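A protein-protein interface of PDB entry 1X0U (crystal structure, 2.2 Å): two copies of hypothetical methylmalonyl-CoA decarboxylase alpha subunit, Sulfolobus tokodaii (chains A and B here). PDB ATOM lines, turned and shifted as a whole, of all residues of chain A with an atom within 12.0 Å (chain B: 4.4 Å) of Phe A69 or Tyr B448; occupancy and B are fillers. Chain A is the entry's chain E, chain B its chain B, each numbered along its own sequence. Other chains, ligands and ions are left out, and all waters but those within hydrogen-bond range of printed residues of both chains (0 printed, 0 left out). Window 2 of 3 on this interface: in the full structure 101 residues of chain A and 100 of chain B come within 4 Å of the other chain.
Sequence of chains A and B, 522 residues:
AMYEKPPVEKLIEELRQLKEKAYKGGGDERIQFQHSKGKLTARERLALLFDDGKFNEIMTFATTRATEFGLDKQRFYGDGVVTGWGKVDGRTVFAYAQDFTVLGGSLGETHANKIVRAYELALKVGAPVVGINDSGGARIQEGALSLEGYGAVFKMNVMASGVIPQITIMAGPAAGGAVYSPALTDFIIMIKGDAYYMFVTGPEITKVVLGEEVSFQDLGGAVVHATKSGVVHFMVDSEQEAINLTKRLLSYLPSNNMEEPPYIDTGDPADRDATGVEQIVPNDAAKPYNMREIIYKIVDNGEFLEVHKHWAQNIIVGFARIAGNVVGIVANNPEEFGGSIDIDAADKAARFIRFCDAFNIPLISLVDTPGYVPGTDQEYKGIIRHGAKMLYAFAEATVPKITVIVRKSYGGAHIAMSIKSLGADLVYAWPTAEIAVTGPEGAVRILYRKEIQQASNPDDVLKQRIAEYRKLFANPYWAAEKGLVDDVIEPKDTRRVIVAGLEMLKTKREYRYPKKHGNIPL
Printed residues of chain B that touch a printed residue of chain A: Ile B446, Leu B447, Tyr B448 and Phe B473.
Printed residues of chain A that touch a printed residue of chain B: Glu A68, Phe A69, Ile A140 and Gln A141.
Hydrophobic or aromatic side chains of chain A that line the printed part of chain B: Phe A69 and Ile A140.
Among the printed residues, no Asp or Glu carboxylate lies within 4 Å of a Lys or Arg side-chain nitrogen of the other chain.
Of the printed residues of chain B, Phe A69 touches Leu B447, Tyr B448 and Phe B473.
No residue of chain A comes within 4 Å of Val B444.
Ile B446 touches just one residue of chain A: Ile A140.
No residue of chain A comes within 4 Å of Arg B449.
No residue of chain A comes within 4 Å of Lys B450.
Glu B451 touches none of the printed residues of chain A.
Ile B452 touches none of the printed residues of chain A.
Printed residues of chain B within 4 Å of Gln A141: Leu B447.
Printed residues of chain B within 4 Å of Glu A68: Phe B473 (3.4 Å).
The nearest printed residue of chain B that does not touch Phe A69 is Val B444 (6.4 Å).
The nearest printed residue of chain B that does not touch Glu A68 is Leu B447 (7.8 Å).
No position is printed for both chains.
Among the printed residues, pairs that only touch across the chains: Ile A140 with Ile B446 (3.0 Å), Phe A69 with Tyr B448 (3.2 Å), Ile A140 with Leu B447 (3.2 Å), Glu A68 with Phe B473 (3.4 Å), Phe A69 with Phe B473 (3.4 Å), Phe A69 with Leu B447 (3.7 Å) and Gln A141 with Leu B447 (3.8 Å).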
ATOM      1  N   THR A  64      18.129   6.899   4.096  1.00  0.00           N
ATOM      2  CA  THR A  64      18.856   5.741   3.598  1.00  0.00           C
ATOM      3  C   THR A  64      18.861   4.679   4.689  1.00  0.00           C
ATOM      4  O   THR A  64      18.832   5.000   5.874  1.00  0.00           O
ATOM      5  CB  THR A  64      20.314   6.069   3.267  1.00  0.00           C
ATOM      6  OG1 THR A  64      20.983   4.864   2.880  1.00  0.00           O
ATOM      7  CG2 THR A  64      21.029   6.668   4.489  1.00  0.00           C
ATOM      8  N   ARG A  65      18.887   3.419   4.276  1.00  0.00           N
ATOM      9  CA  ARG A  65      18.924   2.296   5.196  1.00  0.00           C
ATOM     10  C   ARG A  65      20.298   1.656   5.062  1.00  0.00           C
ATOM     11  O   ARG A  65      20.602   0.663   5.721  1.00  0.00           O
ATOM     12  CB  ARG A  65      17.860   1.265   4.827  1.00  0.00           C
ATOM     13  CG  ARG A  65      16.436   1.792   4.842  1.00  0.00           C
ATOM     14  CD  ARG A  65      15.486   0.673   4.523  1.00  0.00           C
ATOM     15  NE  ARG A  65      14.137   1.143   4.233  1.00  0.00           N
ATOM     16  CZ  ARG A  65      13.142   0.342   3.865  1.00  0.00           C
ATOM     17  NH1 ARG A  65      13.354  -0.961   3.749  1.00  0.00           N
ATOM     18  NH2 ARG A  65      11.940   0.842   3.606  1.00  0.00           N
ATOM     19  N   ALA A  66      21.121   2.229   4.189  1.00  0.00           N
ATOM     20  CA  ALA A  66      22.463   1.716   3.953  1.00  0.00           C
ATOM     21  C   ALA A  66      23.281   1.893   5.216  1.00  0.00           C
ATOM     22  O   ALA A  66      23.091   2.858   5.951  1.00  0.00           O
ATOM     23  CB  ALA A  66      23.122   2.465   2.799  1.00  0.00           C
ATOM     24  N   THR A  67      24.201   0.970   5.463  1.00  0.00           N
ATOM     25  CA  THR A  67      25.024   1.059   6.656  1.00  0.00           C
ATOM     26  C   THR A  67      26.523   1.115   6.370  1.00  0.00           C
ATOM     27  O   THR A  67      27.316   1.398   7.270  1.00  0.00           O
ATOM     28  CB  THR A  67      24.739  -0.122   7.611  1.00  0.00           C
ATOM     29  OG1 THR A  67      25.975  -0.729   7.997  1.00  0.00           O
ATOM     30  CG2 THR A  67      23.850  -1.162   6.936  1.00  0.00           C
ATOM     31  N   GLU A  68      26.910   0.868   5.123  1.00  0.00           N
ATOM     32  CA  GLU A  68      28.321   0.879   4.750  1.00  0.00           C
ATOM     33  C   GLU A  68      28.892   2.262   4.435  1.00  0.00           C
ATOM     34  O   GLU A  68      28.161   3.183   4.072  1.00  0.00           O
ATOM     35  CB  GLU A  68      28.544  -0.075   3.569  1.00  0.00           C
ATOM     36  CG  GLU A  68      28.532  -1.556   3.970  1.00  0.00           C
ATOM     37  CD  GLU A  68      28.650  -2.506   2.785  1.00  0.00           C
ATOM     38  OE1 GLU A  68      28.853  -3.720   3.015  1.00  0.00           O
ATOM     39  OE2 GLU A  68      28.535  -2.049   1.628  1.00  0.00           O
ATOM     40  N   PHE A  69      30.209   2.391   4.587  1.00  0.00           N
ATOM     41  CA  PHE A  69      30.933   3.637   4.334  1.00  0.00           C
ATOM     42  C   PHE A  69      30.369   4.831   5.087  1.00  0.00           C
ATOM     43  O   PHE A  69      30.268   5.938   4.552  1.00  0.00           O
ATOM     44  CB  PHE A  69      30.976   3.949   2.838  1.00  0.00           C
ATOM     45  CG  PHE A  69      31.833   3.005   2.049  1.00  0.00           C
ATOM     46  CD1 PHE A  69      31.365   1.744   1.699  1.00  0.00           C
ATOM     47  CD2 PHE A  69      33.127   3.363   1.689  1.00  0.00           C
ATOM     48  CE1 PHE A  69      32.170   0.860   0.989  1.00  0.00           C
ATOM     49  CE2 PHE A  69      33.940   2.489   0.981  1.00  0.00           C
ATOM     50  CZ  PHE A  69      33.462   1.231   0.636  1.00  0.00           C
ATOM     51  N   GLY A  70      30.004   4.600   6.341  1.00  0.00           N
ATOM     52  CA  GLY A  70      29.467   5.670   7.151  1.00  0.00           C
ATOM     53  C   GLY A  70      28.197   6.244   6.563  1.00  0.00           C
ATOM     54  O   GLY A  70      28.185   7.372   6.084  1.00  0.00           O
ATOM     55  N   LEU A  71      27.130   5.456   6.580  1.00  0.00           N
ATOM     56  CA  LEU A  71      25.831   5.894   6.082  1.00  0.00           C
ATOM     57  C   LEU A  71      24.841   5.656   7.224  1.00  0.00           C
ATOM     58  O   LEU A  71      23.703   6.144   7.210  1.00  0.00           O
ATOM     59  CB  LEU A  71      25.414   5.076   4.849  1.00  0.00           C
ATOM     60  CG  LEU A  71      25.935   5.427   3.444  1.00  0.00           C
ATOM     61  CD1 LEU A  71      25.139   6.587   2.858  1.00  0.00           C
ATOM     62  CD2 LEU A  71      27.416   5.777   3.503  1.00  0.00           C
ATOM     63  N   ASP A  72      25.303   4.894   8.212  1.00  0.00           N
ATOM     64  CA  ASP A  72      24.506   4.540   9.383  1.00  0.00           C
ATOM     65  C   ASP A  72      24.299   5.687  10.357  1.00  0.00           C
ATOM     66  O   ASP A  72      23.356   5.651  11.151  1.00  0.00           O
ATOM     67  CB  ASP A  72      25.159   3.375  10.134  1.00  0.00           C
ATOM     68  CG  ASP A  72      26.637   3.615  10.419  1.00  0.00           C
ATOM     69  OD1 ASP A  72      27.070   4.788  10.423  1.00  0.00           O
ATOM     70  OD2 ASP A  72      27.356   2.625  10.650  1.00  0.00           O
ATOM     71  N   LYS A  73      25.177   6.690  10.312  1.00  0.00           N
ATOM     72  CA  LYS A  73      25.074   7.827  11.220  1.00  0.00           C
ATOM     73  C   LYS A  73      24.599   9.135  10.581  1.00  0.00           C
ATOM     74  O   LYS A  73      23.863   9.904  11.214  1.00  0.00           O
ATOM     75  CB  LYS A  73      26.406   8.040  11.968  1.00  0.00           C
ATOM     76  CG  LYS A  73      27.687   7.705  11.194  1.00  0.00           C
ATOM     77  CD  LYS A  73      27.960   8.664  10.044  1.00  0.00           C
ATOM     78  CE  LYS A  73      27.311   8.187   8.758  1.00  0.00           C
ATOM     79  NZ  LYS A  73      27.515   9.170   7.659  1.00  0.00           N
ATOM     80  N   GLN A  74      25.003   9.400   9.340  1.00  0.00           N
ATOM     81  CA  GLN A  74      24.555  10.619   8.678  1.00  0.00           C
ATOM     82  C   GLN A  74      23.443  10.274   7.703  1.00  0.00           C
ATOM     83  O   GLN A  74      23.690   9.807   6.587  1.00  0.00           O
ATOM     84  CB  GLN A  74      25.700  11.322   7.937  1.00  0.00           C
ATOM     85  CG  GLN A  74      25.249  12.535   7.118  1.00  0.00           C
ATOM     86  CD  GLN A  74      24.225  13.408   7.849  1.00  0.00           C
ATOM     87  OE1 GLN A  74      23.083  12.992   8.081  1.00  0.00           O
ATOM     88  NE2 GLN A  74      24.634  14.622   8.217  1.00  0.00           N
ATOM     89  N   ARG A  75      22.210  10.491   8.148  1.00  0.00           N
ATOM     90  CA  ARG A  75      21.048  10.211   7.328  1.00  0.00           C
ATOM     91  C   ARG A  75      20.188  11.458   7.209  1.00  0.00           C
ATOM     92  O   ARG A  75      19.536  11.886   8.166  1.00  0.00           O
ATOM     93  CB  ARG A  75      20.258   9.045   7.928  1.00  0.00           C
ATOM     94  CG  ARG A  75      21.124   7.811   8.084  1.00  0.00           C
ATOM     95  CD  ARG A  75      20.330   6.564   8.344  1.00  0.00           C
ATOM     96  NE  ARG A  75      21.125   5.375   8.051  1.00  0.00           N
ATOM     97  CZ  ARG A  75      20.707   4.133   8.261  1.00  0.00           C
ATOM     98  NH1 ARG A  75      21.491   3.105   7.964  1.00  0.00           N
ATOM     99  NH2 ARG A  75      19.503   3.921   8.772  1.00  0.00           N
ATOM    100  N   PHE A  76      20.216  12.050   6.024  1.00  0.00           N
ATOM    101  CA  PHE A  76      19.446  13.250   5.745  1.00  0.00           C
ATOM    102  C   PHE A  76      18.012  12.863   5.410  1.00  0.00           C
ATOM    103  O   PHE A  76      17.782  11.960   4.610  1.00  0.00           O
ATOM    104  CB  PHE A  76      20.069  13.984   4.559  1.00  0.00           C
ATOM    105  CG  PHE A  76      21.378  14.649   4.870  1.00  0.00           C
ATOM    106  CD1 PHE A  76      21.413  15.867   5.544  1.00  0.00           C
ATOM    107  CD2 PHE A  76      22.579  14.074   4.459  1.00  0.00           C
ATOM    108  CE1 PHE A  76      22.633  16.508   5.802  1.00  0.00           C
ATOM    109  CE2 PHE A  76      23.807  14.704   4.712  1.00  0.00           C
ATOM    110  CZ  PHE A  76      23.834  15.921   5.380  1.00  0.00           C
ATOM    111  N   ASP A  79      16.515  11.583   1.839  1.00  0.00           N
ATOM    112  CA  ASP A  79      17.616  10.926   1.133  1.00  0.00           C
ATOM    113  C   ASP A  79      18.181  11.611  -0.119  1.00  0.00           C
ATOM    114  O   ASP A  79      18.802  10.956  -0.955  1.00  0.00           O
ATOM    115  CB  ASP A  79      17.241   9.491   0.772  1.00  0.00           C
ATOM    116  CG  ASP A  79      18.462   8.622   0.543  1.00  0.00           C
ATOM    117  OD1 ASP A  79      18.361   7.603  -0.162  1.00  0.00           O
ATOM    118  OD2 ASP A  79      19.534   8.960   1.084  1.00  0.00           O
ATOM    119  N   LEU A 103      24.688  14.740  -0.055  1.00  0.00           N
ATOM    120  CA  LEU A 103      25.623  13.798  -0.671  1.00  0.00           C
ATOM    121  C   LEU A 103      25.665  13.998  -2.190  1.00  0.00           C
ATOM    122  O   LEU A 103      25.426  13.069  -2.970  1.00  0.00           O
ATOM    123  CB  LEU A 103      25.227  12.359  -0.324  1.00  0.00           C
ATOM    124  CG  LEU A 103      25.158  12.021   1.175  1.00  0.00           C
ATOM    125  CD1 LEU A 103      24.681  10.581   1.361  1.00  0.00           C
ATOM    126  CD2 LEU A 103      26.529  12.213   1.826  1.00  0.00           C
ATOM    127  N   SER A 106      23.474  12.492  -4.964  1.00  0.00           N
ATOM    128  CA  SER A 106      23.690  11.149  -5.485  1.00  0.00           C
ATOM    129  C   SER A 106      22.421  10.302  -5.402  1.00  0.00           C
ATOM    130  O   SER A 106      21.535  10.579  -4.591  1.00  0.00           O
ATOM    131  CB  SER A 106      24.829  10.475  -4.721  1.00  0.00           C
ATOM    132  OG  SER A 106      24.507  10.340  -3.349  1.00  0.00           O
ATOM    133  N   ALA A 138      25.514   8.000  -9.242  1.00  0.00           N
ATOM    134  CA  ALA A 138      25.223   6.928  -8.303  1.00  0.00           C
ATOM    135  C   ALA A 138      25.851   7.210  -6.949  1.00  0.00           C
ATOM    136  O   ALA A 138      26.848   7.927  -6.850  1.00  0.00           O
ATOM    137  CB  ALA A 138      25.740   5.608  -8.846  1.00  0.00           C
ATOM    138  N   ARG A 139      25.260   6.669  -5.894  1.00  0.00           N
ATOM    139  CA  ARG A 139      25.846   6.859  -4.582  1.00  0.00           C
ATOM    140  C   ARG A 139      26.791   5.679  -4.462  1.00  0.00           C
ATOM    141  O   ARG A 139      26.362   4.556  -4.205  1.00  0.00           O
ATOM    142  CB  ARG A 139      24.790   6.809  -3.476  1.00  0.00           C
ATOM    143  CG  ARG A 139      25.378   7.112  -2.095  1.00  0.00           C
ATOM    144  CD  ARG A 139      24.295   7.351  -1.070  1.00  0.00           C
ATOM    145  NE  ARG A 139      23.466   8.502  -1.413  1.00  0.00           N
ATOM    146  CZ  ARG A 139      22.280   8.747  -0.867  1.00  0.00           C
ATOM    147  NH1 ARG A 139      21.798   7.914   0.039  1.00  0.00           N
ATOM    148  NH2 ARG A 139      21.583   9.820  -1.221  1.00  0.00           N
ATOM    149  N   ILE A 140      28.075   5.932  -4.675  1.00  0.00           N
ATOM    150  CA  ILE A 140      29.055   4.869  -4.622  1.00  0.00           C
ATOM    151  C   ILE A 140      29.034   4.137  -3.289  1.00  0.00           C
ATOM    152  O   ILE A 140      29.267   2.933  -3.244  1.00  0.00           O
ATOM    153  CB  ILE A 140      30.465   5.409  -4.926  1.00  0.00           C
ATOM    154  CG1 ILE A 140      30.421   6.203  -6.228  1.00  0.00           C
ATOM    155  CG2 ILE A 140      31.455   4.256  -5.085  1.00  0.00           C
ATOM    156  CD1 ILE A 140      31.774   6.496  -6.797  1.00  0.00           C
ATOM    157  N   GLN A 141      28.724   4.853  -2.213  1.00  0.00           N
ATOM    158  CA  GLN A 141      28.663   4.238  -0.887  1.00  0.00           C
ATOM    159  C   GLN A 141      27.630   3.101  -0.799  1.00  0.00           C
ATOM    160  O   GLN A 141      27.715   2.251   0.089  1.00  0.00           O
ATOM    161  CB  GLN A 141      28.369   5.303   0.185  1.00  0.00           C
ATOM    162  CG  GLN A 141      29.452   6.382   0.303  1.00  0.00           C
ATOM    163  CD  GLN A 141      29.198   7.601  -0.585  1.00  0.00           C
ATOM    164  OE1 GLN A 141      28.792   7.477  -1.742  1.00  0.00           O
ATOM    165  NE2 GLN A 141      29.449   8.789  -0.042  1.00  0.00           N
ATOM    166  N   GLU A 142      26.668   3.068  -1.720  1.00  0.00           N
ATOM    167  CA  GLU A 142      25.662   2.012  -1.698  1.00  0.00           C
ATOM    168  C   GLU A 142      25.865   0.930  -2.761  1.00  0.00           C
ATOM    169  O   GLU A 142      25.014   0.069  -2.961  1.00  0.00           O
ATOM    170  CB  GLU A 142      24.258   2.619  -1.793  1.00  0.00           C
ATOM    171  CG  GLU A 142      23.877   3.419  -0.543  1.00  0.00           C
ATOM    172  CD  GLU A 142      22.422   3.852  -0.525  1.00  0.00           C
ATOM    173  OE1 GLU A 142      22.099   4.786   0.229  1.00  0.00           O
ATOM    174  OE2 GLU A 142      21.595   3.252  -1.249  1.00  0.00           O
ATOM    175  N   GLY A 143      27.009   0.980  -3.434  1.00  0.00           N
ATOM    176  CA  GLY A 143      27.348  -0.012  -4.441  1.00  0.00           C
ATOM    177  C   GLY A 143      26.309  -0.406  -5.478  1.00  0.00           C
ATOM    178  O   GLY A 143      25.714   0.451  -6.137  1.00  0.00           O
ATOM    179  N   ALA A 144      26.089  -1.713  -5.614  1.00  0.00           N
ATOM    180  CA  ALA A 144      25.153  -2.254  -6.605  1.00  0.00           C
ATOM    181  C   ALA A 144      23.692  -1.897  -6.353  1.00  0.00           C
ATOM    182  O   ALA A 144      22.881  -1.900  -7.273  1.00  0.00           O
ATOM    183  CB  ALA A 144      25.311  -3.766  -6.692  1.00  0.00           C
ATOM    184  N   LEU A 145      23.359  -1.610  -5.103  1.00  0.00           N
ATOM    185  CA  LEU A 145      22.000  -1.234  -4.746  1.00  0.00           C
ATOM    186  C   LEU A 145      21.665   0.092  -5.423  1.00  0.00           C
ATOM    187  O   LEU A 145      20.517   0.349  -5.776  1.00  0.00           O
ATOM    188  CB  LEU A 145      21.887  -1.094  -3.224  1.00  0.00           C
ATOM    189  CG  LEU A 145      21.224  -2.224  -2.445  1.00  0.00           C
ATOM    190  CD1 LEU A 145      21.313  -3.527  -3.202  1.00  0.00           C
ATOM    191  CD2 LEU A 145      21.886  -2.338  -1.081  1.00  0.00           C
ATOM    192  N   SER A 146      22.680   0.930  -5.607  1.00  0.00           N
ATOM    193  CA  SER A 146      22.479   2.221  -6.252  1.00  0.00           C
ATOM    194  C   SER A 146      22.139   2.012  -7.731  1.00  0.00           C
ATOM    195  O   SER A 146      21.269   2.696  -8.277  1.00  0.00           O
ATOM    196  CB  SER A 146      23.734   3.084  -6.104  1.00  0.00           C
ATOM    197  OG  SER A 146      23.516   4.387  -6.611  1.00  0.00           O
ATOM    198  N   VAL B 444      36.945   3.769  -5.487  1.00  0.00           N
ATOM    199  CA  VAL B 444      37.755   4.198  -4.354  1.00  0.00           C
ATOM    200  C   VAL B 444      38.456   5.519  -4.624  1.00  0.00           C
ATOM    201  O   VAL B 444      38.718   6.304  -3.713  1.00  0.00           O
ATOM    202  CB  VAL B 444      38.834   3.162  -4.019  1.00  0.00           C
ATOM    203  CG1 VAL B 444      38.202   1.803  -3.785  1.00  0.00           C
ATOM    204  CG2 VAL B 444      39.851   3.104  -5.140  1.00  0.00           C
ATOM    205  N   ILE B 446      37.415   7.994  -5.363  1.00  0.00           N
ATOM    206  CA  ILE B 446      36.537   9.105  -5.017  1.00  0.00           C
ATOM    207  C   ILE B 446      35.818   8.818  -3.698  1.00  0.00           C
ATOM    208  O   ILE B 446      35.076   9.653  -3.183  1.00  0.00           O
ATOM    209  CB  ILE B 446      35.514   9.419  -6.137  1.00  0.00           C
ATOM    210  CG1 ILE B 446      34.205   8.691  -5.906  1.00  0.00           C
ATOM    211  CG2 ILE B 446      36.071   9.006  -7.488  1.00  0.00           C
ATOM    212  CD1 ILE B 446      33.133   9.193  -6.827  1.00  0.00           C
ATOM    213  N   LEU B 447      36.055   7.632  -3.149  1.00  0.00           N
ATOM    214  CA  LEU B 447      35.465   7.227  -1.875  1.00  0.00           C
ATOM    215  C   LEU B 447      36.504   7.606  -0.825  1.00  0.00           C
ATOM    216  O   LEU B 447      36.171   8.002   0.298  1.00  0.00           O
ATOM    217  CB  LEU B 447      35.255   5.709  -1.857  1.00  0.00           C
ATOM    218  CG  LEU B 447      33.885   5.054  -1.627  1.00  0.00           C
ATOM    219  CD1 LEU B 447      32.757   6.080  -1.558  1.00  0.00           C
ATOM    220  CD2 LEU B 447      33.649   4.080  -2.758  1.00  0.00           C
ATOM    221  N   TYR B 448      37.772   7.476  -1.218  1.00  0.00           N
ATOM    222  CA  TYR B 448      38.899   7.774  -0.346  1.00  0.00           C
ATOM    223  C   TYR B 448      39.753   8.906  -0.893  1.00  0.00           C
ATOM    224  O   TYR B 448      40.964   8.954  -0.672  1.00  0.00           O
ATOM    225  CB  TYR B 448      39.742   6.513  -0.155  1.00  0.00           C
ATOM    226  CG  TYR B 448      38.976   5.380   0.479  1.00  0.00           C
ATOM    227  CD1 TYR B 448      39.474   4.077   0.454  1.00  0.00           C
ATOM    228  CD2 TYR B 448      37.750   5.606   1.111  1.00  0.00           C
ATOM    229  CE1 TYR B 448      38.765   3.026   1.042  1.00  0.00           C
ATOM    230  CE2 TYR B 448      37.038   4.565   1.699  1.00  0.00           C
ATOM    231  CZ  TYR B 448      37.548   3.282   1.660  1.00  0.00           C
ATOM    232  OH  TYR B 448      36.841   2.246   2.223  1.00  0.00           O
ATOM    233  N   ARG B 449      39.109   9.820  -1.611  1.00  0.00           N
ATOM    234  CA  ARG B 449      39.805  10.970  -2.163  1.00  0.00           C
ATOM    235  C   ARG B 449      40.441  11.685  -0.965  1.00  0.00           C
ATOM    236  O   ARG B 449      41.422  12.419  -1.103  1.00  0.00           O
ATOM    237  CB  ARG B 449      38.810  11.912  -2.853  1.00  0.00           C
ATOM    238  CG  ARG B 449      39.379  12.734  -4.008  1.00  0.00           C
ATOM    239  CD  ARG B 449      40.855  13.074  -3.823  1.00  0.00           C
ATOM    240  NE  ARG B 449      41.729  11.944  -4.137  1.00  0.00           N
ATOM    241  CZ  ARG B 449      43.058  11.981  -4.080  1.00  0.00           C
ATOM    242  NH1 ARG B 449      43.765  10.901  -4.390  1.00  0.00           N
ATOM    243  NH2 ARG B 449      43.682  13.091  -3.704  1.00  0.00           N
ATOM    244  N   LYS B 450      39.870  11.457   0.218  1.00  0.00           N
ATOM    245  CA  LYS B 450      40.367  12.070   1.449  1.00  0.00           C
ATOM    246  C   LYS B 450      40.937  11.065   2.453  1.00  0.00           C
ATOM    247  O   LYS B 450      40.626  11.100   3.650  1.00  0.00           O
ATOM    248  CB  LYS B 450      39.255  12.898   2.101  1.00  0.00           C
ATOM    249  CG  LYS B 450      39.323  14.406   1.825  1.00  0.00           C
ATOM    250  CD  LYS B 450      39.748  14.732   0.391  1.00  0.00           C
ATOM    251  CE  LYS B 450      41.231  15.116   0.293  1.00  0.00           C
ATOM    252  NZ  LYS B 450      42.170  14.019   0.666  1.00  0.00           N
ATOM    253  N   GLU B 451      41.787  10.178   1.950  1.00  0.00           N
ATOM    254  CA  GLU B 451      42.425   9.164   2.772  1.00  0.00           C
ATOM    255  C   GLU B 451      43.648   8.694   2.007  1.00  0.00           C
ATOM    256  O   GLU B 451      44.259   7.675   2.339  1.00  0.00           O
ATOM    257  CB  GLU B 451      41.481   7.981   3.014  1.00  0.00           C
ATOM    258  CG  GLU B 451      42.016   6.960   4.021  1.00  0.00           C
ATOM    259  CD  GLU B 451      41.147   5.714   4.129  1.00  0.00           C
ATOM    260  OE1 GLU B 451      41.210   4.854   3.220  1.00  0.00           O
ATOM    261  OE2 GLU B 451      40.401   5.599   5.125  1.00  0.00           O
ATOM    262  N   ILE B 452      43.998   9.452   0.974  1.00  0.00           N
ATOM    263  CA  ILE B 452      45.146   9.116   0.144  1.00  0.00           C
ATOM    264  C   ILE B 452      46.462   9.543   0.795  1.00  0.00           C
ATOM    265  O   ILE B 452      47.309   8.700   1.091  1.00  0.00           O
ATOM    266  CB  ILE B 452      45.005   9.742  -1.296  1.00  0.00           C
ATOM    267  CG1 ILE B 452      46.090  10.797  -1.551  1.00  0.00           C
ATOM    268  CG2 ILE B 452      43.622  10.346  -1.450  1.00  0.00           C
ATOM    269  CD1 ILE B 452      46.198  11.263  -2.993  1.00  0.00           C
ATOM    270  N   GLN B 464      44.512  -1.494   1.028  1.00  0.00           N
ATOM    271  CA  GLN B 464      43.341  -1.010   1.762  1.00  0.00           C
ATOM    272  C   GLN B 464      42.238  -0.364   0.901  1.00  0.00           C
ATOM    273  O   GLN B 464      41.140  -0.108   1.408  1.00  0.00           O
ATOM    274  CB  GLN B 464      43.802  -0.033   2.857  1.00  0.00           C
ATOM    275  CG  GLN B 464      42.694   0.530   3.750  1.00  0.00           C
ATOM    276  CD  GLN B 464      42.595   2.052   3.677  1.00  0.00           C
ATOM    277  OE1 GLN B 464      42.189   2.611   2.656  1.00  0.00           O
ATOM    278  NE2 GLN B 464      42.973   2.725   4.760  1.00  0.00           N
ATOM    279  N   ARG B 465      42.510  -0.121  -0.388  1.00  0.00           N
ATOM    280  CA  ARG B 465      41.513   0.503  -1.275  1.00  0.00           C
ATOM    281  C   ARG B 465      40.985  -0.356  -2.446  1.00  0.00           C
ATOM    282  O   ARG B 465      40.027  -1.104  -2.262  1.00  0.00           O
ATOM    283  CB  ARG B 465      42.038   1.849  -1.809  1.00  0.00           C
ATOM    284  CG  ARG B 465      43.026   1.745  -2.967  1.00  0.00           C
ATOM    285  CD  ARG B 465      44.263   0.985  -2.550  1.00  0.00           C
ATOM    286  NE  ARG B 465      44.727   0.031  -3.555  1.00  0.00           N
ATOM    287  CZ  ARG B 465      44.440  -1.269  -3.560  1.00  0.00           C
ATOM    288  NH1 ARG B 465      44.923  -2.053  -4.519  1.00  0.00           N
ATOM    289  NH2 ARG B 465      43.679  -1.787  -2.604  1.00  0.00           N
ATOM    290  N   PHE B 473      33.844  -6.184  -2.685  1.00  0.00           N
ATOM    291  CA  PHE B 473      32.687  -5.977  -3.549  1.00  0.00           C
ATOM    292  C   PHE B 473      32.771  -6.609  -4.937  1.00  0.00           C
ATOM    293  O   PHE B 473      31.743  -6.954  -5.521  1.00  0.00           O
ATOM    294  CB  PHE B 473      32.423  -4.479  -3.697  1.00  0.00           C
ATOM    295  CG  PHE B 473      32.273  -3.759  -2.391  1.00  0.00           C
ATOM    296  CD1 PHE B 473      33.328  -3.024  -1.860  1.00  0.00           C
ATOM    297  CD2 PHE B 473      31.075  -3.809  -1.694  1.00  0.00           C
ATOM    298  CE1 PHE B 473      33.188  -2.343  -0.653  1.00  0.00           C
ATOM    299  CE2 PHE B 473      30.922  -3.133  -0.489  1.00  0.00           C
ATOM    300  CZ  PHE B 473      31.981  -2.398   0.035  1.00  0.00           C
